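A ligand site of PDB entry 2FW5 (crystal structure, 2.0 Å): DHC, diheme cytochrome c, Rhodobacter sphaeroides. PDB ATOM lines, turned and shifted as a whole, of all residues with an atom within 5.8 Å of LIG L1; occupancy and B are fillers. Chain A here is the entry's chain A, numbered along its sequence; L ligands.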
ATOM      1  N   LEU A  13      19.363  -7.129  25.569  1.00  0.00           N
ATOM      2  CA  LEU A  13      17.941  -7.354  25.574  1.00  0.00           C
ATOM      3  C   LEU A  13      17.505  -7.381  24.112  1.00  0.00           C
ATOM      4  O   LEU A  13      16.802  -6.494  23.633  1.00  0.00           O
ATOM      5  CB  LEU A  13      17.220  -6.263  26.370  1.00  0.00           C
ATOM      6  CG  LEU A  13      17.397  -6.320  27.889  1.00  0.00           C
ATOM      7  CD1 LEU A  13      16.578  -5.252  28.520  1.00  0.00           C
ATOM      8  CD2 LEU A  13      17.005  -7.671  28.467  1.00  0.00           C
ATOM      9  N   MET A  29       7.177  -6.215  18.085  1.00  0.00           N
ATOM     10  CA  MET A  29       8.597  -6.534  18.244  1.00  0.00           C
ATOM     11  C   MET A  29       8.776  -7.920  18.830  1.00  0.00           C
ATOM     12  O   MET A  29       7.928  -8.367  19.649  1.00  0.00           O
ATOM     13  CB  MET A  29       9.256  -5.500  19.210  1.00  0.00           C
ATOM     14  CG  MET A  29      10.786  -5.538  19.267  1.00  0.00           C
ATOM     15  SD  MET A  29      11.248  -4.393  20.556  1.00  0.00           S
ATOM     16  CE  MET A  29      11.462  -5.368  22.056  1.00  0.00           C
ATOM     17  N   TYR A  31       9.992  -9.906  21.381  1.00  0.00           N
ATOM     18  CA  TYR A  31      10.458  -9.620  22.738  1.00  0.00           C
ATOM     19  C   TYR A  31      11.618 -10.542  23.212  1.00  0.00           C
ATOM     20  O   TYR A  31      11.572 -11.761  23.053  1.00  0.00           O
ATOM     21  CB  TYR A  31       9.319  -9.717  23.716  1.00  0.00           C
ATOM     22  CG  TYR A  31       8.124  -8.899  23.362  1.00  0.00           C
ATOM     23  CD1 TYR A  31       6.891  -9.524  22.997  1.00  0.00           C
ATOM     24  CD2 TYR A  31       8.184  -7.526  23.397  1.00  0.00           C
ATOM     25  CE1 TYR A  31       5.759  -8.749  22.681  1.00  0.00           C
ATOM     26  CE2 TYR A  31       7.066  -6.743  23.054  1.00  0.00           C
ATOM     27  CZ  TYR A  31       5.854  -7.362  22.695  1.00  0.00           C
ATOM     28  OH  TYR A  31       4.746  -6.559  22.397  1.00  0.00           O
ATOM     29  N   PRO A  32      12.638  -9.922  23.827  1.00  0.00           N
ATOM     30  CA  PRO A  32      13.799 -10.642  24.374  1.00  0.00           C
ATOM     31  C   PRO A  32      13.435 -11.709  25.483  1.00  0.00           C
ATOM     32  O   PRO A  32      12.677 -11.380  26.392  1.00  0.00           O
ATOM     33  CB  PRO A  32      14.627  -9.531  25.037  1.00  0.00           C
ATOM     34  CG  PRO A  32      14.110  -8.256  24.473  1.00  0.00           C
ATOM     35  CD  PRO A  32      12.705  -8.480  24.065  1.00  0.00           C
ATOM     36  N   LEU A  35      13.190 -11.195  29.436  1.00  0.00           N
ATOM     37  CA  LEU A  35      12.181 -10.415  30.115  1.00  0.00           C
ATOM     38  C   LEU A  35      11.008 -11.235  30.760  1.00  0.00           C
ATOM     39  O   LEU A  35      10.175 -10.642  31.419  1.00  0.00           O
ATOM     40  CB  LEU A  35      11.671  -9.372  29.146  1.00  0.00           C
ATOM     41  CG  LEU A  35      12.324  -7.976  29.167  1.00  0.00           C
ATOM     42  CD1 LEU A  35      13.665  -7.763  29.973  1.00  0.00           C
ATOM     43  CD2 LEU A  35      12.291  -7.342  27.757  1.00  0.00           C
ATOM     44  N   ARG A  82      16.935  -9.188  36.115  1.00  0.00           N
ATOM     45  CA  ARG A  82      16.304  -8.017  36.701  1.00  0.00           C
ATOM     46  C   ARG A  82      14.809  -8.089  36.576  1.00  0.00           C
ATOM     47  O   ARG A  82      14.082  -7.661  37.478  1.00  0.00           O
ATOM     48  CB  ARG A  82      16.826  -6.779  36.010  1.00  0.00           C
ATOM     49  CG  ARG A  82      16.603  -6.709  34.499  1.00  0.00           C
ATOM     50  CD  ARG A  82      16.646  -5.293  33.958  1.00  0.00           C
ATOM     51  NE  ARG A  82      17.411  -5.156  32.717  1.00  0.00           N
ATOM     52  CZ  ARG A  82      17.684  -3.962  32.149  1.00  0.00           C
ATOM     53  NH1 ARG A  82      17.249  -2.808  32.698  1.00  0.00           N
ATOM     54  NH2 ARG A  82      18.374  -3.916  31.017  1.00  0.00           N
ATOM     55  N   ILE A  96       4.996  -9.112  29.687  1.00  0.00           N
ATOM     56  CA  ILE A  96       6.133  -8.336  30.176  1.00  0.00           C
ATOM     57  C   ILE A  96       5.584  -7.029  30.761  1.00  0.00           C
ATOM     58  O   ILE A  96       6.057  -6.583  31.814  1.00  0.00           O
ATOM     59  CB  ILE A  96       7.076  -8.015  28.984  1.00  0.00           C
ATOM     60  CG1 ILE A  96       7.723  -9.317  28.491  1.00  0.00           C
ATOM     61  CG2 ILE A  96       8.068  -6.940  29.361  1.00  0.00           C
ATOM     62  CD1 ILE A  96       8.538  -9.211  27.158  1.00  0.00           C
ATOM     63  N   SER A  97       4.598  -6.408  30.095  1.00  0.00           N
ATOM     64  CA  SER A  97       4.096  -5.111  30.568  1.00  0.00           C
ATOM     65  C   SER A  97       3.306  -5.174  31.919  1.00  0.00           C
ATOM     66  O   SER A  97       2.920  -4.138  32.425  1.00  0.00           O
ATOM     67  CB  SER A  97       3.230  -4.409  29.512  1.00  0.00           C
ATOM     68  OG  SER A  97       2.162  -5.271  29.092  1.00  0.00           O
ATOM     69  N   TRP A 101       8.497  -5.336  37.924  1.00  0.00           N
ATOM     70  CA  TRP A 101       9.734  -4.666  37.510  1.00  0.00           C
ATOM     71  C   TRP A 101       9.493  -3.662  36.358  1.00  0.00           C
ATOM     72  O   TRP A 101      10.020  -2.516  36.383  1.00  0.00           O
ATOM     73  CB  TRP A 101      10.792  -5.712  37.126  1.00  0.00           C
ATOM     74  CG  TRP A 101      11.902  -5.148  36.316  1.00  0.00           C
ATOM     75  CD1 TRP A 101      13.061  -4.492  36.807  1.00  0.00           C
ATOM     76  CD2 TRP A 101      11.994  -5.105  34.886  1.00  0.00           C
ATOM     77  NE1 TRP A 101      13.833  -4.107  35.745  1.00  0.00           N
ATOM     78  CE2 TRP A 101      13.214  -4.459  34.560  1.00  0.00           C
ATOM     79  CE3 TRP A 101      11.149  -5.563  33.818  1.00  0.00           C
ATOM     80  CZ2 TRP A 101      13.616  -4.260  33.226  1.00  0.00           C
ATOM     81  CZ3 TRP A 101      11.555  -5.357  32.496  1.00  0.00           C
ATOM     82  CH2 TRP A 101      12.798  -4.720  32.218  1.00  0.00           C
ATOM     83  N   PHE A 102       8.659  -4.060  35.379  1.00  0.00           N
ATOM     84  CA  PHE A 102       8.275  -3.200  34.262  1.00  0.00           C
ATOM     85  C   PHE A 102       7.493  -1.963  34.734  1.00  0.00           C
ATOM     86  O   PHE A 102       7.790  -0.846  34.337  1.00  0.00           O
ATOM     87  CB  PHE A 102       7.433  -4.006  33.211  1.00  0.00           C
ATOM     88  CG  PHE A 102       7.085  -3.219  31.946  1.00  0.00           C
ATOM     89  CD1 PHE A 102       7.866  -3.360  30.780  1.00  0.00           C
ATOM     90  CD2 PHE A 102       5.941  -2.419  31.897  1.00  0.00           C
ATOM     91  CE1 PHE A 102       7.528  -2.654  29.608  1.00  0.00           C
ATOM     92  CE2 PHE A 102       5.597  -1.711  30.692  1.00  0.00           C
ATOM     93  CZ  PHE A 102       6.381  -1.869  29.569  1.00  0.00           C
ATOM     94  N   LYS A 105       9.776   0.565  36.435  1.00  0.00           N
ATOM     95  CA  LYS A 105      10.573   1.322  35.459  1.00  0.00           C
ATOM     96  C   LYS A 105       9.736   2.325  34.654  1.00  0.00           C
ATOM     97  O   LYS A 105      10.307   3.273  34.152  1.00  0.00           O
ATOM     98  CB  LYS A 105      11.346   0.416  34.456  1.00  0.00           C
ATOM     99  CG  LYS A 105      12.311  -0.669  35.044  1.00  0.00           C
ATOM    100  CD  LYS A 105      13.568  -0.108  35.809  1.00  0.00           C
ATOM    101  N   HIS A 106       8.425   2.108  34.482  1.00  0.00           N
ATOM    102  CA  HIS A 106       7.571   2.971  33.636  1.00  0.00           C
ATOM    103  C   HIS A 106       6.641   3.970  34.368  1.00  0.00           C
ATOM    104  O   HIS A 106       6.111   4.907  33.753  1.00  0.00           O
ATOM    105  CB  HIS A 106       6.744   2.121  32.639  1.00  0.00           C
ATOM    106  CG  HIS A 106       7.615   1.524  31.574  1.00  0.00           C
ATOM    107  ND1 HIS A 106       8.313   0.351  31.768  1.00  0.00           N
ATOM    108  CD2 HIS A 106       8.017   2.029  30.389  1.00  0.00           C
ATOM    109  CE1 HIS A 106       9.091   0.134  30.714  1.00  0.00           C
ATOM    110  NE2 HIS A 106       8.919   1.135  29.852  1.00  0.00           N
ATOM    111  N   GLU A 109       7.235   7.715  34.545  1.00  0.00           N
ATOM    112  CA  GLU A 109       7.962   8.077  33.334  1.00  0.00           C
ATOM    113  C   GLU A 109       7.073   8.269  32.083  1.00  0.00           C
ATOM    114  O   GLU A 109       7.442   8.969  31.137  1.00  0.00           O
ATOM    115  CB  GLU A 109       9.029   7.013  33.067  1.00  0.00           C
ATOM    116  CG  GLU A 109       9.889   6.721  34.315  1.00  0.00           C
ATOM    117  CD  GLU A 109      11.045   7.721  34.486  1.00  0.00           C
ATOM    118  OE1 GLU A 109      11.191   8.649  33.620  1.00  0.00           O
ATOM    119  OE2 GLU A 109      11.843   7.552  35.492  1.00  0.00           O
ATOM    120  N   VAL A 110       5.909   7.630  32.092  1.00  0.00           N
ATOM    121  CA  VAL A 110       4.978   7.704  30.939  1.00  0.00           C
ATOM    122  C   VAL A 110       3.755   8.583  31.184  1.00  0.00           C
ATOM    123  O   VAL A 110       2.961   8.332  32.068  1.00  0.00           O
ATOM    124  CB  VAL A 110       4.545   6.279  30.491  1.00  0.00           C
ATOM    125  CG1 VAL A 110       3.583   6.369  29.288  1.00  0.00           C
ATOM    126  CG2 VAL A 110       5.739   5.410  30.165  1.00  0.00           C
ATOM    127  N   MET A 114       2.235  10.519  26.010  1.00  0.00           N
ATOM    128  CA  MET A 114       3.186   9.534  25.484  1.00  0.00           C
ATOM    129  C   MET A 114       2.483   8.173  25.283  1.00  0.00           C
ATOM    130  O   MET A 114       2.691   7.500  24.293  1.00  0.00           O
ATOM    131  CB  MET A 114       4.362   9.308  26.431  1.00  0.00           C
ATOM    132  CG  MET A 114       5.268  10.459  26.650  1.00  0.00           C
ATOM    133  SD  MET A 114       6.354   9.931  28.058  1.00  0.00           S
ATOM    134  CE  MET A 114       7.012   8.409  27.204  1.00  0.00           C
ATOM    135  N   LEU A 115       1.645   7.784  26.242  1.00  0.00           N
ATOM    136  CA  LEU A 115       0.949   6.526  26.142  1.00  0.00           C
ATOM    137  C   LEU A 115      -0.070   6.494  24.958  1.00  0.00           C
ATOM    138  O   LEU A 115      -0.174   5.508  24.239  1.00  0.00           O
ATOM    139  CB  LEU A 115       0.262   6.208  27.492  1.00  0.00           C
ATOM    140  CG  LEU A 115      -0.571   4.915  27.507  1.00  0.00           C
ATOM    141  CD1 LEU A 115       0.232   3.661  27.113  1.00  0.00           C
ATOM    142  CD2 LEU A 115      -1.307   4.730  28.900  1.00  0.00           C
ATOM    143  N   ALA A 118       1.891   5.839  21.769  1.00  0.00           N
ATOM    144  CA  ALA A 118       2.382   4.449  21.664  1.00  0.00           C
ATOM    145  C   ALA A 118       1.274   3.441  21.329  1.00  0.00           C
ATOM    146  O   ALA A 118       1.572   2.386  20.745  1.00  0.00           O
ATOM    147  CB  ALA A 118       3.103   4.005  22.959  1.00  0.00           C
ATOM    148  N   SER A 120      -0.136   1.255  22.983  1.00  0.00           N
ATOM    149  CA  SER A 120      -0.085   0.143  23.930  1.00  0.00           C
ATOM    150  C   SER A 120       1.322   0.146  24.537  1.00  0.00           C
ATOM    151  O   SER A 120       2.284   0.457  23.808  1.00  0.00           O
ATOM    152  CB  SER A 120      -0.291  -1.197  23.207  1.00  0.00           C
ATOM    153  OG  SER A 120      -0.134  -2.237  24.146  1.00  0.00           O
ATOM    154  N   MET A 121       1.443  -0.192  25.819  1.00  0.00           N
ATOM    155  CA  MET A 121       2.782  -0.452  26.436  1.00  0.00           C
ATOM    156  C   MET A 121       3.494  -1.664  25.820  1.00  0.00           C
ATOM    157  O   MET A 121       4.661  -1.833  26.037  1.00  0.00           O
ATOM    158  CB  MET A 121       2.668  -0.691  27.967  1.00  0.00           C
ATOM    159  CG  MET A 121       2.277   0.555  28.720  1.00  0.00           C
ATOM    160  SD  MET A 121       3.351   2.028  28.355  1.00  0.00           S
ATOM    161  CE  MET A 121       5.080   1.479  28.897  1.00  0.00           C
ATOM    162  N   SER A 122       2.748  -2.544  25.075  1.00  0.00           N
ATOM    163  CA  SER A 122       3.356  -3.586  24.237  1.00  0.00           C
ATOM    164  C   SER A 122       4.221  -3.104  23.082  1.00  0.00           C
ATOM    165  O   SER A 122       5.034  -3.843  22.546  1.00  0.00           O
ATOM    166  CB  SER A 122       2.212  -4.492  23.647  1.00  0.00           C
ATOM    167  OG  SER A 122       1.409  -4.976  24.716  1.00  0.00           O
ATOM    168  N   ASN A 123       4.041  -1.859  22.676  1.00  0.00           N
ATOM    169  CA  ASN A 123       4.689  -1.280  21.504  1.00  0.00           C
ATOM    170  C   ASN A 123       6.009  -0.560  21.846  1.00  0.00           C
ATOM    171  O   ASN A 123       6.041   0.682  21.752  1.00  0.00           O
ATOM    172  CB  ASN A 123       3.692  -0.267  20.924  1.00  0.00           C
ATOM    173  CG  ASN A 123       2.411  -0.965  20.396  1.00  0.00           C
ATOM    174  OD1 ASN A 123       2.395  -2.169  20.236  1.00  0.00           O
ATOM    175  ND2 ASN A 123       1.347  -0.185  20.173  1.00  0.00           N
ATOM    176  N   CYS A 124       7.047  -1.305  22.261  1.00  0.00           N
ATOM    177  CA  CYS A 124       8.254  -0.746  22.865  1.00  0.00           C
ATOM    178  C   CYS A 124       8.981   0.256  21.952  1.00  0.00           C
ATOM    179  O   CYS A 124       9.443   1.341  22.405  1.00  0.00           O
ATOM    180  CB  CYS A 124       9.259  -1.856  23.193  1.00  0.00           C
ATOM    181  SG  CYS A 124       8.596  -3.426  23.839  1.00  0.00           S
ATOM    182  N   ALA A 126       7.758   2.186  19.731  1.00  0.00           N
ATOM    183  CA  ALA A 126       7.150   3.494  19.559  1.00  0.00           C
ATOM    184  C   ALA A 126       7.781   4.527  20.517  1.00  0.00           C
ATOM    185  O   ALA A 126       7.723   5.740  20.250  1.00  0.00           O
ATOM    186  CB  ALA A 126       5.580   3.475  19.664  1.00  0.00           C
ATOM    187  N   CYS A 127       8.399   4.047  21.613  1.00  0.00           N
ATOM    188  CA  CYS A 127       8.968   4.943  22.610  1.00  0.00           C
ATOM    189  C   CYS A 127      10.460   4.797  22.724  1.00  0.00           C
ATOM    190  O   CYS A 127      11.100   5.721  23.200  1.00  0.00           O
ATOM    191  CB  CYS A 127       8.373   4.753  24.002  1.00  0.00           C
ATOM    192  SG  CYS A 127       6.636   5.172  24.068  1.00  0.00           S
ATOM    193  N   HIS A 128      10.993   3.629  22.370  1.00  0.00           N
ATOM    194  CA  HIS A 128      12.407   3.340  22.498  1.00  0.00           C
ATOM    195  C   HIS A 128      12.959   3.112  21.085  1.00  0.00           C
ATOM    196  O   HIS A 128      12.782   1.999  20.538  1.00  0.00           O
ATOM    197  CB  HIS A 128      12.600   2.059  23.291  1.00  0.00           C
ATOM    198  CG  HIS A 128      12.122   2.103  24.707  1.00  0.00           C
ATOM    199  ND1 HIS A 128      12.832   2.725  25.701  1.00  0.00           N
ATOM    200  CD2 HIS A 128      11.067   1.513  25.302  1.00  0.00           C
ATOM    201  CE1 HIS A 128      12.210   2.551  26.857  1.00  0.00           C
ATOM    202  NE2 HIS A 128      11.131   1.815  26.647  1.00  0.00           N
ATOM    203  N   PHE A 136      17.265   0.542  25.572  1.00  0.00           N
ATOM    204  CA  PHE A 136      16.012   1.053  26.178  1.00  0.00           C
ATOM    205  C   PHE A 136      16.157   2.279  27.086  1.00  0.00           C
ATOM    206  O   PHE A 136      17.313   2.717  27.337  1.00  0.00           O
ATOM    207  CB  PHE A 136      15.345  -0.057  26.989  1.00  0.00           C
ATOM    208  CG  PHE A 136      14.873  -1.199  26.167  1.00  0.00           C
ATOM    209  CD1 PHE A 136      15.672  -2.335  25.985  1.00  0.00           C
ATOM    210  CD2 PHE A 136      13.607  -1.143  25.530  1.00  0.00           C
ATOM    211  CE1 PHE A 136      15.191  -3.422  25.194  1.00  0.00           C
ATOM    212  CE2 PHE A 136      13.145  -2.210  24.797  1.00  0.00           C
ATOM    213  CZ  PHE A 136      13.934  -3.317  24.604  1.00  0.00           C
HETATM  214 FE1  LIG L   1      10.028   1.445  28.291  1.00  0.00          FE
HETATM  215  C1  LIG L   1      12.150   2.707  30.453  1.00  0.00           C
HETATM  216  C2  LIG L   1      11.786  -1.654  28.377  1.00  0.00           C
HETATM  217  C3  LIG L   1       7.681   0.030  26.349  1.00  0.00           C
HETATM  218  C4  LIG L   1       8.586   4.596  27.726  1.00  0.00           C
HETATM  219  N1  LIG L   1      11.663   0.625  29.210  1.00  0.00           N
HETATM  220  C5  LIG L   1      12.402   1.379  30.104  1.00  0.00           C
HETATM  221  C6  LIG L   1      13.464   0.539  30.616  1.00  0.00           C
HETATM  222  C7  LIG L   1      13.403  -0.656  30.026  1.00  0.00           C
HETATM  223  C8  LIG L   1      12.241  -0.638  29.157  1.00  0.00           C
HETATM  224  C9  LIG L   1      14.311  -1.912  30.256  1.00  0.00           C
HETATM  225  C10 LIG L   1      14.539   1.002  31.647  1.00  0.00           C
HETATM  226  C11 LIG L   1      15.744   1.593  30.918  1.00  0.00           C
HETATM  227  C12 LIG L   1      16.881   1.774  31.944  1.00  0.00           C
HETATM  228  O1  LIG L   1      17.672   0.818  32.248  1.00  0.00           O
HETATM  229  O2  LIG L   1      16.989   2.915  32.473  1.00  0.00           O
HETATM  230  N2  LIG L   1       9.784  -0.445  27.503  1.00  0.00           N
HETATM  231  C13 LIG L   1      10.593  -1.573  27.668  1.00  0.00           C
HETATM  232  C14 LIG L   1       9.986  -2.663  26.903  1.00  0.00           C
HETATM  233  C15 LIG L   1       8.808  -2.220  26.392  1.00  0.00           C
HETATM  234  C16 LIG L   1       8.691  -0.792  26.732  1.00  0.00           C
HETATM  235  C17 LIG L   1      10.551  -4.096  26.849  1.00  0.00           C
HETATM  236  C18 LIG L   1       7.793  -3.058  25.560  1.00  0.00           C
HETATM  237  C19 LIG L   1       7.257  -4.252  26.020  1.00  0.00           C
HETATM  238  N3  LIG L   1       8.440   2.179  27.236  1.00  0.00           N
HETATM  239  C20 LIG L   1       7.593   1.382  26.486  1.00  0.00           C
HETATM  240  C21 LIG L   1       6.592   2.228  25.867  1.00  0.00           C
HETATM  241  C22 LIG L   1       6.836   3.489  26.284  1.00  0.00           C
HETATM  242  C23 LIG L   1       8.034   3.481  27.101  1.00  0.00           C
HETATM  243  C24 LIG L   1       5.413   1.765  24.962  1.00  0.00           C
HETATM  244  C25 LIG L   1       6.037   4.779  25.930  1.00  0.00           C
HETATM  245  C26 LIG L   1       4.690   4.930  26.129  1.00  0.00           C
HETATM  246  N4  LIG L   1      10.292   3.397  28.963  1.00  0.00           N
HETATM  247  C27 LIG L   1       9.605   4.527  28.603  1.00  0.00           C
HETATM  248  C28 LIG L   1      10.181   5.640  29.298  1.00  0.00           C
HETATM  249  C29 LIG L   1      11.296   5.043  30.128  1.00  0.00           C
HETATM  250  C30 LIG L   1      11.294   3.631  29.869  1.00  0.00           C
HETATM  251  C31 LIG L   1       9.717   7.091  29.132  1.00  0.00           C
HETATM  252  C32 LIG L   1      12.234   5.783  31.100  1.00  0.00           C
HETATM  253  C33 LIG L   1      13.454   6.246  30.370  1.00  0.00           C
HETATM  254  C34 LIG L   1      14.285   6.802  31.480  1.00  0.00           C
HETATM  255  O3  LIG L   1      13.748   7.047  32.616  1.00  0.00           O
HETATM  256  O4  LIG L   1      15.479   6.992  31.199  1.00  0.00           O
HETATM  257 FE1  LG2 L   2       2.488 -11.846  20.512  1.00  0.00          FE
HETATM  258  C1  LG2 L   2       1.386  -9.690  22.912  1.00  0.00           C
HETATM  259  C2  LG2 L   2       4.939 -13.020  22.654  1.00  0.00           C
HETATM  260  C3  LG2 L   2       3.782 -13.802  17.979  1.00  0.00           C
HETATM  261  C4  LG2 L   2      -0.128 -10.864  18.356  1.00  0.00           C
HETATM  262  N1  LG2 L   2       3.064 -11.413  22.502  1.00  0.00           N
HETATM  263  C5  LG2 L   2       2.474 -10.474  23.256  1.00  0.00           C
HETATM  264  C6  LG2 L   2       3.158 -10.487  24.549  1.00  0.00           C
HETATM  265  C7  LG2 L   2       4.140 -11.390  24.473  1.00  0.00           C
HETATM  266  C8  LG2 L   2       4.096 -12.005  23.162  1.00  0.00           C
HETATM  267  C9  LG2 L   2       5.163 -11.772  25.567  1.00  0.00           C
HETATM  268  C10 LG2 L   2       2.756  -9.541  25.745  1.00  0.00           C
HETATM  269  C11 LG2 L   2       3.344  -8.194  25.359  1.00  0.00           C
HETATM  270  C12 LG2 L   2       3.216  -7.327  26.651  1.00  0.00           C
HETATM  271  O1  LG2 L   2       3.949  -7.538  27.627  1.00  0.00           O
HETATM  272  O2  LG2 L   2       2.369  -6.429  26.746  1.00  0.00           O
HETATM  273  N2  LG2 L   2       4.096 -13.162  20.360  1.00  0.00           N
HETATM  274  C13 LG2 L   2       4.916 -13.545  21.395  1.00  0.00           C
HETATM  275  C14 LG2 L   2       5.766 -14.582  20.889  1.00  0.00           C
HETATM  276  C15 LG2 L   2       5.463 -14.805  19.603  1.00  0.00           C
HETATM  277  C16 LG2 L   2       4.396 -13.907  19.237  1.00  0.00           C
HETATM  278  C17 LG2 L   2       6.790 -15.275  21.803  1.00  0.00           C
HETATM  279  C18 LG2 L   2       6.054 -15.877  18.644  1.00  0.00           C
HETATM  280  C19 LG2 L   2       5.783 -17.212  18.852  1.00  0.00           C
HETATM  281  N3  LG2 L   2       1.923 -12.271  18.506  1.00  0.00           N
HETATM  282  C20 LG2 L   2       2.650 -13.070  17.661  1.00  0.00           C
HETATM  283  C21 LG2 L   2       1.975 -13.021  16.362  1.00  0.00           C
HETATM  284  C22 LG2 L   2       0.866 -12.206  16.471  1.00  0.00           C
HETATM  285  C23 LG2 L   2       0.835 -11.722  17.838  1.00  0.00           C
HETATM  286  C24 LG2 L   2       2.520 -13.788  15.153  1.00  0.00           C
HETATM  287  C25 LG2 L   2      -0.216 -11.770  15.425  1.00  0.00           C
HETATM  288  C26 LG2 L   2      -0.853 -12.711  14.636  1.00  0.00           C
HETATM  289  N4  LG2 L   2       0.848 -10.520  20.593  1.00  0.00           N
HETATM  290  C27 LG2 L   2      -0.098 -10.254  19.589  1.00  0.00           C
HETATM  291  C28 LG2 L   2      -1.072  -9.288  20.067  1.00  0.00           C
HETATM  292  C29 LG2 L   2      -0.600  -8.926  21.481  1.00  0.00           C
HETATM  293  C30 LG2 L   2       0.609  -9.712  21.736  1.00  0.00           C
HETATM  294  C31 LG2 L   2      -2.307  -8.723  19.295  1.00  0.00           C
HETATM  295  C32 LG2 L   2      -1.290  -7.889  22.399  1.00  0.00           C
HETATM  296  C33 LG2 L   2      -0.501  -6.570  22.258  1.00  0.00           C
HETATM  297  C34 LG2 L   2      -1.168  -5.481  23.122  1.00  0.00           C
HETATM  298  O3  LG2 L   2      -1.767  -5.779  24.196  1.00  0.00           O
HETATM  299  O4  LG2 L   2      -1.099  -4.304  22.724  1.00  0.00           O
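OH of Tyr 31 sits at hydrogen-bond distance from O of Ser 122. OG of Ser 120 sits at hydrogen-bond distance from N of Ser 122, 3.0 Å away. ND2 of Asn 123 lies close to N of Ser 120 (3.5 Å). ND1 of His 106 sits at hydrogen-bond distance from O of Phe 102 (2.9 Å). The side-chain amide nitrogen (ND2) of Asn 123 sits at hydrogen-bond distance from the backbone carbonyl oxygen (O) of Ala 118 (2.6 Å).
O3 of LIG L1 lies close to OE1 of Glu 109 (3.2 Å). Residues that only touch LIG L1: Met 121, Phe 136, Asn 123, Phe 102, Met 114, Ser 120, Val 110, Ala 118, Trp 101, Leu 35 and Tyr 31. Hydrophobic or aromatic side chains within 4 Å of LIG L1: Tyr 31, Leu 35, Trp 101, Phe 102, His 106, Val 110, Met 114, Ala 118, Met 121, His 128 and Phe 136. 17 residues have an atom within 4 Å of LIG L1: Tyr 31, Leu 35, Arg 82, Trp 101, Phe 102, His 106, Glu 109, Val 110, Met 114, Ala 118, Ser 120, Met 121, Asn 123, Cys 124, Cys 127, His 128 and Phe 136.
O1 of LG2 L2 is in hydrogen-bond range of N of Ser 97, 2.8 Å away. The side-chain hydroxyl (OG) of Ser 97 lies within hydrogen-bond range of an oxygen (O2) of LG2 L2, 2.6 Å away. A carbon (C25) of LIG L1 is covalently linked to the side-chain sulfur of Cys 127, 2.0 Å away. O1 of LG2 L2 sits at hydrogen-bond distance from N of Ile 96 (2.8 Å). SG of Cys 124 is covalently linked to C18 of LIG L1 (1.9 Å). NH1 of Arg 82 lies within salt-bridge range of O1 of LIG L1, 3.7 Å away. OG of Ser 122 is in hydrogen-bond range of O2 of LG2 L2 (2.7 Å). NE2 of His 128 is bound to FE1 of LIG L1, at 2.0 Å. A ring nitrogen (NE2) of His 106 is bound to an iron atom (FE1) of LIG L1 (1.9 Å). The side-chain hydroxyl (OG) of Ser 120 lies within hydrogen-bond range of an oxygen (O4) of LG2 L2 (2.7 Å).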
